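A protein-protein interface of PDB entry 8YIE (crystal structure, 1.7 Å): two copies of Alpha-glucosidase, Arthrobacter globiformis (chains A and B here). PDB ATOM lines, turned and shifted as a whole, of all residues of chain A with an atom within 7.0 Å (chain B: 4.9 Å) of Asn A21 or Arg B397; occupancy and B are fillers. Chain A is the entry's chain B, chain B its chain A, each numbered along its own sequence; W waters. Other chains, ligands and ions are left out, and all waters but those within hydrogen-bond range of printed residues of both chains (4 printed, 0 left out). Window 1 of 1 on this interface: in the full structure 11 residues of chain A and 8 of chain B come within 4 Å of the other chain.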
ATOM      1  N   ARG A  18     -27.872  26.514  -7.206  1.00  0.00           N
ATOM      2  CA  ARG A  18     -28.502  26.510  -5.887  1.00  0.00           C
ATOM      3  C   ARG A  18     -27.435  26.391  -4.807  1.00  0.00           C
ATOM      4  O   ARG A  18     -26.544  25.542  -4.904  1.00  0.00           O
ATOM      5  CB  ARG A  18     -29.508  25.365  -5.750  1.00  0.00           C
ATOM      6  CG  ARG A  18     -30.647  25.664  -4.795  1.00  0.00           C
ATOM      7  CD  ARG A  18     -31.778  24.690  -5.018  1.00  0.00           C
ATOM      8  NE  ARG A  18     -32.522  24.429  -3.790  1.00  0.00           N
ATOM      9  CZ  ARG A  18     -33.675  25.004  -3.485  1.00  0.00           C
ATOM     10  NH1 ARG A  18     -34.234  25.898  -4.286  1.00  0.00           N
ATOM     11  NH2 ARG A  18     -34.287  24.671  -2.353  1.00  0.00           N
ATOM     12  N   ASP A  19     -27.577  27.203  -3.759  1.00  0.00           N
ATOM     13  CA  ASP A  19     -26.575  27.395  -2.701  1.00  0.00           C
ATOM     14  C   ASP A  19     -27.118  26.841  -1.373  1.00  0.00           C
ATOM     15  O   ASP A  19     -27.882  27.512  -0.671  1.00  0.00           O
ATOM     16  CB  ASP A  19     -26.242  28.886  -2.628  1.00  0.00           C
ATOM     17  CG  ASP A  19     -25.430  29.267  -1.415  1.00  0.00           C
ATOM     18  OD1 ASP A  19     -24.702  28.418  -0.876  1.00  0.00           O
ATOM     19  OD2 ASP A  19     -25.511  30.446  -1.014  1.00  0.00           O
ATOM     20  N   ALA A  20     -26.695  25.623  -1.022  1.00  0.00           N
ATOM     21  CA  ALA A  20     -27.275  24.912   0.120  1.00  0.00           C
ATOM     22  C   ALA A  20     -26.811  25.444   1.474  1.00  0.00           C
ATOM     23  O   ALA A  20     -27.544  25.313   2.460  1.00  0.00           O
ATOM     24  CB  ALA A  20     -26.963  23.412   0.031  1.00  0.00           C
ATOM     25  N   ASN A  21     -25.616  26.020   1.574  1.00  0.00           N
ATOM     26  CA  ASN A  21     -25.138  26.490   2.874  1.00  0.00           C
ATOM     27  C   ASN A  21     -25.143  28.008   3.013  1.00  0.00           C
ATOM     28  O   ASN A  21     -24.710  28.526   4.049  1.00  0.00           O
ATOM     29  CB  ASN A  21     -23.737  25.934   3.174  1.00  0.00           C
ATOM     30  CG  ASN A  21     -22.666  26.600   2.351  1.00  0.00           C
ATOM     31  OD1 ASN A  21     -22.907  26.923   1.193  1.00  0.00           O
ATOM     32  ND2 ASN A  21     -21.481  26.824   2.935  1.00  0.00           N
ATOM     33  N   GLY A  22     -25.626  28.742   2.016  1.00  0.00           N
ATOM     34  CA  GLY A  22     -25.803  30.170   2.208  1.00  0.00           C
ATOM     35  C   GLY A  22     -24.547  31.022   2.194  1.00  0.00           C
ATOM     36  O   GLY A  22     -24.559  32.132   2.748  1.00  0.00           O
ATOM     37  N   ASP A  23     -23.467  30.573   1.552  1.00  0.00           N
ATOM     38  CA  ASP A  23     -22.275  31.401   1.424  1.00  0.00           C
ATOM     39  C   ASP A  23     -22.213  32.156   0.092  1.00  0.00           C
ATOM     40  O   ASP A  23     -21.227  32.854  -0.170  1.00  0.00           O
ATOM     41  CB  ASP A  23     -21.002  30.552   1.631  1.00  0.00           C
ATOM     42  CG  ASP A  23     -20.848  29.447   0.597  1.00  0.00           C
ATOM     43  OD1 ASP A  23     -21.693  29.361  -0.310  1.00  0.00           O
ATOM     44  OD2 ASP A  23     -19.877  28.673   0.698  1.00  0.00           O
ATOM     45  N   GLY A  24     -23.246  32.044  -0.746  1.00  0.00           N
ATOM     46  CA  GLY A  24     -23.323  32.774  -1.998  1.00  0.00           C
ATOM     47  C   GLY A  24     -22.842  32.011  -3.213  1.00  0.00           C
ATOM     48  O   GLY A  24     -22.991  32.505  -4.340  1.00  0.00           O
ATOM     49  N   ILE A  25     -22.261  30.840  -3.016  1.00  0.00           N
ATOM     50  CA  ILE A  25     -21.700  30.015  -4.079  1.00  0.00           C
ATOM     51  C   ILE A  25     -22.581  28.781  -4.245  1.00  0.00           C
ATOM     52  O   ILE A  25     -22.751  27.998  -3.303  1.00  0.00           O
ATOM     53  CB  ILE A  25     -20.262  29.609  -3.732  1.00  0.00           C
ATOM     54  CG1 ILE A  25     -19.365  30.842  -3.651  1.00  0.00           C
ATOM     55  CG2 ILE A  25     -19.741  28.534  -4.686  1.00  0.00           C
ATOM     56  CD1 ILE A  25     -18.064  30.578  -2.911  1.00  0.00           C
ATOM     57  N   GLY A  26     -23.138  28.588  -5.436  1.00  0.00           N
ATOM     58  CA  GLY A  26     -23.892  27.370  -5.683  1.00  0.00           C
ATOM     59  C   GLY A  26     -23.017  26.144  -5.495  1.00  0.00           C
ATOM     60  O   GLY A  26     -21.813  26.196  -5.703  1.00  0.00           O
ATOM     61  N   ASP A  27     -23.625  25.029  -5.077  1.00  0.00           N
ATOM     62  CA  ASP A  27     -22.813  23.890  -4.661  1.00  0.00           C
ATOM     63  C   ASP A  27     -23.527  22.577  -4.986  1.00  0.00           C
ATOM     64  O   ASP A  27     -24.650  22.563  -5.500  1.00  0.00           O
ATOM     65  CB  ASP A  27     -22.475  24.006  -3.167  1.00  0.00           C
ATOM     66  CG  ASP A  27     -23.695  24.345  -2.314  1.00  0.00           C
ATOM     67  OD1 ASP A  27     -24.759  23.782  -2.564  1.00  0.00           O
ATOM     68  OD2 ASP A  27     -23.588  25.164  -1.388  1.00  0.00           O
ATOM     69  N   GLY A  29     -24.595  20.274  -2.822  1.00  0.00           N
ATOM     70  CA  GLY A  29     -25.773  20.077  -1.991  1.00  0.00           C
ATOM     71  C   GLY A  29     -26.984  20.780  -2.570  1.00  0.00           C
ATOM     72  O   GLY A  29     -28.103  20.255  -2.531  1.00  0.00           O
ATOM     73  N   GLY A  30     -26.764  21.963  -3.150  1.00  0.00           N
ATOM     74  CA  GLY A  30     -27.844  22.688  -3.798  1.00  0.00           C
ATOM     75  C   GLY A  30     -28.331  22.004  -5.063  1.00  0.00           C
ATOM     76  O   GLY A  30     -29.533  21.998  -5.347  1.00  0.00           O
ATOM     77  N   GLN A  33     -30.686  19.386  -4.144  1.00  0.00           N
ATOM     78  CA  GLN A  33     -32.013  19.912  -3.829  1.00  0.00           C
ATOM     79  C   GLN A  33     -32.819  20.205  -5.085  1.00  0.00           C
ATOM     80  O   GLN A  33     -34.054  20.152  -5.046  1.00  0.00           O
ATOM     81  CB  GLN A  33     -31.903  21.183  -2.989  1.00  0.00           C
ATOM     82  CG  GLN A  33     -31.307  20.978  -1.601  1.00  0.00           C
ATOM     83  CD  GLN A  33     -31.048  22.291  -0.902  1.00  0.00           C
ATOM     84  OE1 GLN A  33     -31.084  23.351  -1.525  1.00  0.00           O
ATOM     85  NE2 GLN A  33     -30.788  22.228   0.402  1.00  0.00           N
ATOM     86  N   ALA A  72     -15.308  24.511  -2.207  1.00  0.00           N
ATOM     87  CA  ALA A  72     -16.444  25.426  -2.224  1.00  0.00           C
ATOM     88  C   ALA A  72     -17.689  24.788  -2.819  1.00  0.00           C
ATOM     89  O   ALA A  72     -18.791  25.319  -2.640  1.00  0.00           O
ATOM     90  CB  ALA A  72     -16.083  26.698  -3.002  1.00  0.00           C
ATOM     91  N   SER A 431     -30.827  30.629  -2.105  1.00  0.00           N
ATOM     92  CA  SER A 431     -30.369  30.233  -0.782  1.00  0.00           C
ATOM     93  C   SER A 431     -31.353  30.808   0.226  1.00  0.00           C
ATOM     94  O   SER A 431     -32.350  31.430  -0.147  1.00  0.00           O
ATOM     95  CB  SER A 431     -28.972  30.777  -0.517  1.00  0.00           C
ATOM     96  OG  SER A 431     -29.063  32.195  -0.457  1.00  0.00           O
ATOM     97  N   ASP A 432     -31.047  30.635   1.519  1.00  0.00           N
ATOM     98  CA  ASP A 432     -31.799  31.323   2.564  1.00  0.00           C
ATOM     99  C   ASP A 432     -31.045  32.528   3.128  1.00  0.00           C
ATOM    100  O   ASP A 432     -31.425  33.054   4.178  1.00  0.00           O
ATOM    101  CB  ASP A 432     -32.177  30.352   3.691  1.00  0.00           C
ATOM    102  CG  ASP A 432     -30.967  29.818   4.454  1.00  0.00           C
ATOM    103  OD1 ASP A 432     -29.819  30.083   4.038  1.00  0.00           O
ATOM    104  OD2 ASP A 432     -31.170  29.137   5.488  1.00  0.00           O
ATOM    105  N   ALA A 433     -30.018  32.993   2.431  1.00  0.00           N
ATOM    106  CA  ALA A 433     -29.036  33.952   2.925  1.00  0.00           C
ATOM    107  C   ALA A 433     -29.350  35.367   2.429  1.00  0.00           C
ATOM    108  O   ALA A 433     -30.306  35.594   1.684  1.00  0.00           O
ATOM    109  CB  ALA A 433     -27.633  33.528   2.481  1.00  0.00           C
ATOM    110  N   LEU B 390     -11.673  20.966  12.875  1.00  0.00           N
ATOM    111  CA  LEU B 390     -11.250  22.229  12.291  1.00  0.00           C
ATOM    112  C   LEU B 390     -11.184  22.197  10.771  1.00  0.00           C
ATOM    113  O   LEU B 390     -11.195  23.265  10.140  1.00  0.00           O
ATOM    114  CB  LEU B 390      -9.874  22.626  12.840  1.00  0.00           C
ATOM    115  CG  LEU B 390      -9.810  22.992  14.324  1.00  0.00           C
ATOM    116  CD1 LEU B 390      -8.371  22.997  14.820  1.00  0.00           C
ATOM    117  CD2 LEU B 390     -10.498  24.329  14.595  1.00  0.00           C
ATOM    118  N   ASP B 391     -11.112  21.004  10.183  1.00  0.00           N
ATOM    119  CA  ASP B 391     -10.969  20.818   8.739  1.00  0.00           C
ATOM    120  C   ASP B 391     -12.323  20.433   8.144  1.00  0.00           C
ATOM    121  O   ASP B 391     -12.613  19.264   7.884  1.00  0.00           O
ATOM    122  CB  ASP B 391      -9.914  19.754   8.452  1.00  0.00           C
ATOM    123  CG  ASP B 391      -9.588  19.635   6.978  1.00  0.00           C
ATOM    124  OD1 ASP B 391     -10.068  20.475   6.186  1.00  0.00           O
ATOM    125  OD2 ASP B 391      -8.868  18.685   6.609  1.00  0.00           O
ATOM    126  N   LEU B 392     -13.172  21.434   7.958  1.00  0.00           N
ATOM    127  CA  LEU B 392     -14.408  21.267   7.212  1.00  0.00           C
ATOM    128  C   LEU B 392     -14.265  21.959   5.870  1.00  0.00           C
ATOM    129  O   LEU B 392     -13.638  23.021   5.798  1.00  0.00           O
ATOM    130  CB  LEU B 392     -15.612  21.865   7.955  1.00  0.00           C
ATOM    131  CG  LEU B 392     -15.940  21.201   9.292  1.00  0.00           C
ATOM    132  CD1 LEU B 392     -17.016  21.986  10.022  1.00  0.00           C
ATOM    133  CD2 LEU B 392     -16.392  19.783   9.047  1.00  0.00           C
ATOM    134  N   PRO B 393     -14.801  21.389   4.794  1.00  0.00           N
ATOM    135  CA  PRO B 393     -14.796  22.107   3.515  1.00  0.00           C
ATOM    136  C   PRO B 393     -15.672  23.347   3.586  1.00  0.00           C
ATOM    137  O   PRO B 393     -16.632  23.413   4.351  1.00  0.00           O
ATOM    138  CB  PRO B 393     -15.372  21.089   2.527  1.00  0.00           C
ATOM    139  CG  PRO B 393     -16.232  20.208   3.367  1.00  0.00           C
ATOM    140  CD  PRO B 393     -15.554  20.126   4.718  1.00  0.00           C
ATOM    141  N   ASP B 394     -15.344  24.326   2.732  1.00  0.00           N
ATOM    142  CA  ASP B 394     -16.078  25.591   2.729  1.00  0.00           C
ATOM    143  C   ASP B 394     -17.574  25.375   2.539  1.00  0.00           C
ATOM    144  O   ASP B 394     -18.387  26.067   3.165  1.00  0.00           O
ATOM    145  CB  ASP B 394     -15.543  26.510   1.628  1.00  0.00           C
ATOM    146  CG  ASP B 394     -14.122  27.003   1.896  1.00  0.00           C
ATOM    147  OD1 ASP B 394     -13.439  26.472   2.799  1.00  0.00           O
ATOM    148  OD2 ASP B 394     -13.693  27.941   1.191  1.00  0.00           O
ATOM    149  N   ALA B 395     -17.962  24.438   1.659  1.00  0.00           N
ATOM    150  CA  ALA B 395     -19.379  24.205   1.379  1.00  0.00           C
ATOM    151  C   ALA B 395     -20.128  23.592   2.556  1.00  0.00           C
ATOM    152  O   ALA B 395     -21.365  23.612   2.558  1.00  0.00           O
ATOM    153  CB  ALA B 395     -19.545  23.296   0.161  1.00  0.00           C
ATOM    154  N   ALA B 396     -19.417  23.059   3.549  1.00  0.00           N
ATOM    155  CA  ALA B 396     -20.064  22.489   4.727  1.00  0.00           C
ATOM    156  C   ALA B 396     -20.300  23.508   5.833  1.00  0.00           C
ATOM    157  O   ALA B 396     -21.140  23.268   6.715  1.00  0.00           O
ATOM    158  CB  ALA B 396     -19.229  21.330   5.287  1.00  0.00           C
ATOM    159  N   ARG B 397     -19.598  24.632   5.816  1.00  0.00           N
ATOM    160  CA  ARG B 397     -19.733  25.587   6.910  1.00  0.00           C
ATOM    161  C   ARG B 397     -21.087  26.286   6.869  1.00  0.00           C
ATOM    162  O   ARG B 397     -21.543  26.740   5.810  1.00  0.00           O
ATOM    163  CB  ARG B 397     -18.600  26.603   6.853  1.00  0.00           C
ATOM    164  CG  ARG B 397     -17.251  25.917   6.972  1.00  0.00           C
ATOM    165  CD  ARG B 397     -16.278  26.728   7.781  1.00  0.00           C
ATOM    166  NE  ARG B 397     -14.986  26.060   7.874  1.00  0.00           N
ATOM    167  CZ  ARG B 397     -14.535  25.437   8.957  1.00  0.00           C
ATOM    168  NH1 ARG B 397     -15.246  25.385  10.076  1.00  0.00           N
ATOM    169  NH2 ARG B 397     -13.338  24.855   8.916  1.00  0.00           N
ATOM    170  N   GLN B 398     -21.745  26.353   8.035  1.00  0.00           N
ATOM    171  CA  GLN B 398     -23.066  26.953   8.147  1.00  0.00           C
ATOM    172  C   GLN B 398     -23.144  28.099   9.140  1.00  0.00           C
ATOM    173  O   GLN B 398     -24.095  28.887   9.067  1.00  0.00           O
ATOM    174  CB  GLN B 398     -24.101  25.887   8.544  1.00  0.00           C
ATOM    175  CG  GLN B 398     -24.035  24.678   7.646  1.00  0.00           C
ATOM    176  CD  GLN B 398     -25.382  24.202   7.213  1.00  0.00           C
ATOM    177  OE1 GLN B 398     -26.321  24.144   8.017  1.00  0.00           O
ATOM    178  NE2 GLN B 398     -25.515  23.908   5.919  1.00  0.00           N
ATOM    179  N   ASP B 399     -22.198  28.198  10.067  1.00  0.00           N
ATOM    180  CA  ASP B 399     -22.171  29.285  11.036  1.00  0.00           C
ATOM    181  C   ASP B 399     -22.188  30.631  10.312  1.00  0.00           C
ATOM    182  O   ASP B 399     -21.404  30.832   9.375  1.00  0.00           O
ATOM    183  CB  ASP B 399     -20.910  29.128  11.891  1.00  0.00           C
ATOM    184  CG  ASP B 399     -20.854  30.069  13.067  1.00  0.00           C
ATOM    185  OD1 ASP B 399     -21.532  31.103  13.064  1.00  0.00           O
ATOM    186  OD2 ASP B 399     -20.098  29.765  14.009  1.00  0.00           O
ATOM    187  N   TRP B 402     -18.926  32.418   9.462  1.00  0.00           N
ATOM    188  CA  TRP B 402     -18.129  32.082   8.283  1.00  0.00           C
ATOM    189  C   TRP B 402     -18.346  33.087   7.156  1.00  0.00           C
ATOM    190  O   TRP B 402     -17.384  33.669   6.636  1.00  0.00           O
ATOM    191  CB  TRP B 402     -18.456  30.663   7.808  1.00  0.00           C
ATOM    192  CG  TRP B 402     -17.764  30.292   6.505  1.00  0.00           C
ATOM    193  CD1 TRP B 402     -18.349  30.100   5.287  1.00  0.00           C
ATOM    194  CD2 TRP B 402     -16.358  30.074   6.313  1.00  0.00           C
ATOM    195  NE1 TRP B 402     -17.396  29.764   4.350  1.00  0.00           N
ATOM    196  CE2 TRP B 402     -16.166  29.748   4.955  1.00  0.00           C
ATOM    197  CE3 TRP B 402     -15.246  30.117   7.160  1.00  0.00           C
ATOM    198  CZ2 TRP B 402     -14.904  29.473   4.421  1.00  0.00           C
ATOM    199  CZ3 TRP B 402     -13.988  29.849   6.626  1.00  0.00           C
ATOM    200  CH2 TRP B 402     -13.831  29.528   5.270  1.00  0.00           C
ATOM    201  N   LEU B 410     -13.237  30.855  11.281  1.00  0.00           N
ATOM    202  CA  LEU B 410     -13.767  29.528  10.969  1.00  0.00           C
ATOM    203  C   LEU B 410     -15.202  29.381  11.448  1.00  0.00           C
ATOM    204  O   LEU B 410     -16.024  28.766  10.768  1.00  0.00           O
ATOM    205  CB  LEU B 410     -12.910  28.433  11.605  1.00  0.00           C
ATOM    206  CG  LEU B 410     -11.531  28.168  10.996  1.00  0.00           C
ATOM    207  CD1 LEU B 410     -10.926  26.934  11.641  1.00  0.00           C
ATOM    208  CD2 LEU B 410     -11.634  28.006   9.484  1.00  0.00           C
ATOM    209  N   ASP B 413     -18.816  25.536  13.791  1.00  0.00           N
ATOM    210  CA  ASP B 413     -19.365  24.261  13.333  1.00  0.00           C
ATOM    211  C   ASP B 413     -18.555  23.065  13.823  1.00  0.00           C
ATOM    212  O   ASP B 413     -19.115  21.968  13.980  1.00  0.00           O
ATOM    213  CB  ASP B 413     -19.453  24.243  11.801  1.00  0.00           C
ATOM    214  CG  ASP B 413     -20.505  25.214  11.263  1.00  0.00           C
ATOM    215  OD1 ASP B 413     -21.650  25.220  11.765  1.00  0.00           O
ATOM    216  OD2 ASP B 413     -20.181  25.990  10.338  1.00  0.00           O
HETATM  217  O   HOH W   1     -25.952  28.495   6.426  1.00  0.00           O
HETATM  218  O   HOH W   2     -17.461  29.817   1.404  1.00  0.00           O
HETATM  219  O   HOH W   3     -22.205  29.459   5.153  1.00  0.00           O
HETATM  220  O   HOH W   4     -23.234  23.329   0.672  1.00  0.00           O
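Of the 13 printed residues of chain B, 4 touch a printed residue of chain A.
No position is printed for both chains.
Water W4 lies within hydrogen-bond range of the backbone carbonyl oxygen of Ala B395 (2.7 Å) and the side-chain carboxylate of Asp A27 (2.8 Å). Water W1 lies within hydrogen-bond range of O of Asn A21 and O of Gln B398. Water W2 lies within hydrogen-bond range of OD2 of Asp A23 (2.8 Å) and NE1 of Trp B402 (2.9 Å). Water W3 lies within hydrogen-bond range of the backbone carbonyl oxygen of Arg B397 (2.9 Å) and the backbone carbonyl oxygen of Asn A21 (2.9 Å).
The backbone NH (N) of Gln B398 is in hydrogen-bond range of the side-chain carboxylate (OD2) of Asp B413 (2.8 Å). The side-chain carboxylate of Asp A19 lies close to the side-chain amide oxygen of Asn A21. OD1 of Asp A23 lies within hydrogen-bond range of N of Ile A25, 3.1 Å away. OD1 of Asn A21 sits close to OD2 of Asp A27 (3.2 Å). The side-chain amide oxygen (OD1) of Asn A21 lies close to the side-chain carboxylate (OD1) of Asp A23 (3.1 Å). OD2 of Asp A19 sits at hydrogen-bond distance from N of Asp A23, at 3.3 Å.
Asn A21 touches just these residues of chain B: Asp B394, Ala B395, Arg B397 and Gln B398. Arg B397 touches just one residue of chain A: Asn A21. Of the printed residues of chain A, Ala B395 touches Asn A21 and Ala A72. Of the printed residues of chain B, Ala A72 touches Ala B395 (3.5 Å). Of the printed residues of chain B, Asp A23 touches Asp B394. Of the printed residues of chain A, Gln B398 touches Asn A21 (3.8 Å). Printed residues of chain A within 4 Å of Asp B394: Asn A21 and Asp A23. Leu B390 touches none of the printed residues of chain A. Ile A25 touches none of the printed residues of chain B.
The backbone carbonyl oxygen (O) of Ala B395 lies within hydrogen-bond range of the side-chain amide nitrogen (ND2) of Asn A21. The backbone carbonyl oxygen (O) of Asp B394 is in hydrogen-bond range of the side-chain amide nitrogen (ND2) of Asn A21 (3.2 Å). The backbone carbonyl oxygen (O) of Arg B397 sits at hydrogen-bond distance from the side-chain amide nitrogen (ND2) of Asn A21 (2.9 Å).
Asn A21 touches Gln B398. Asp B394 touches Asp A23. Ala B395 touches Ala A72 (CB to O, 3.5 Å).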
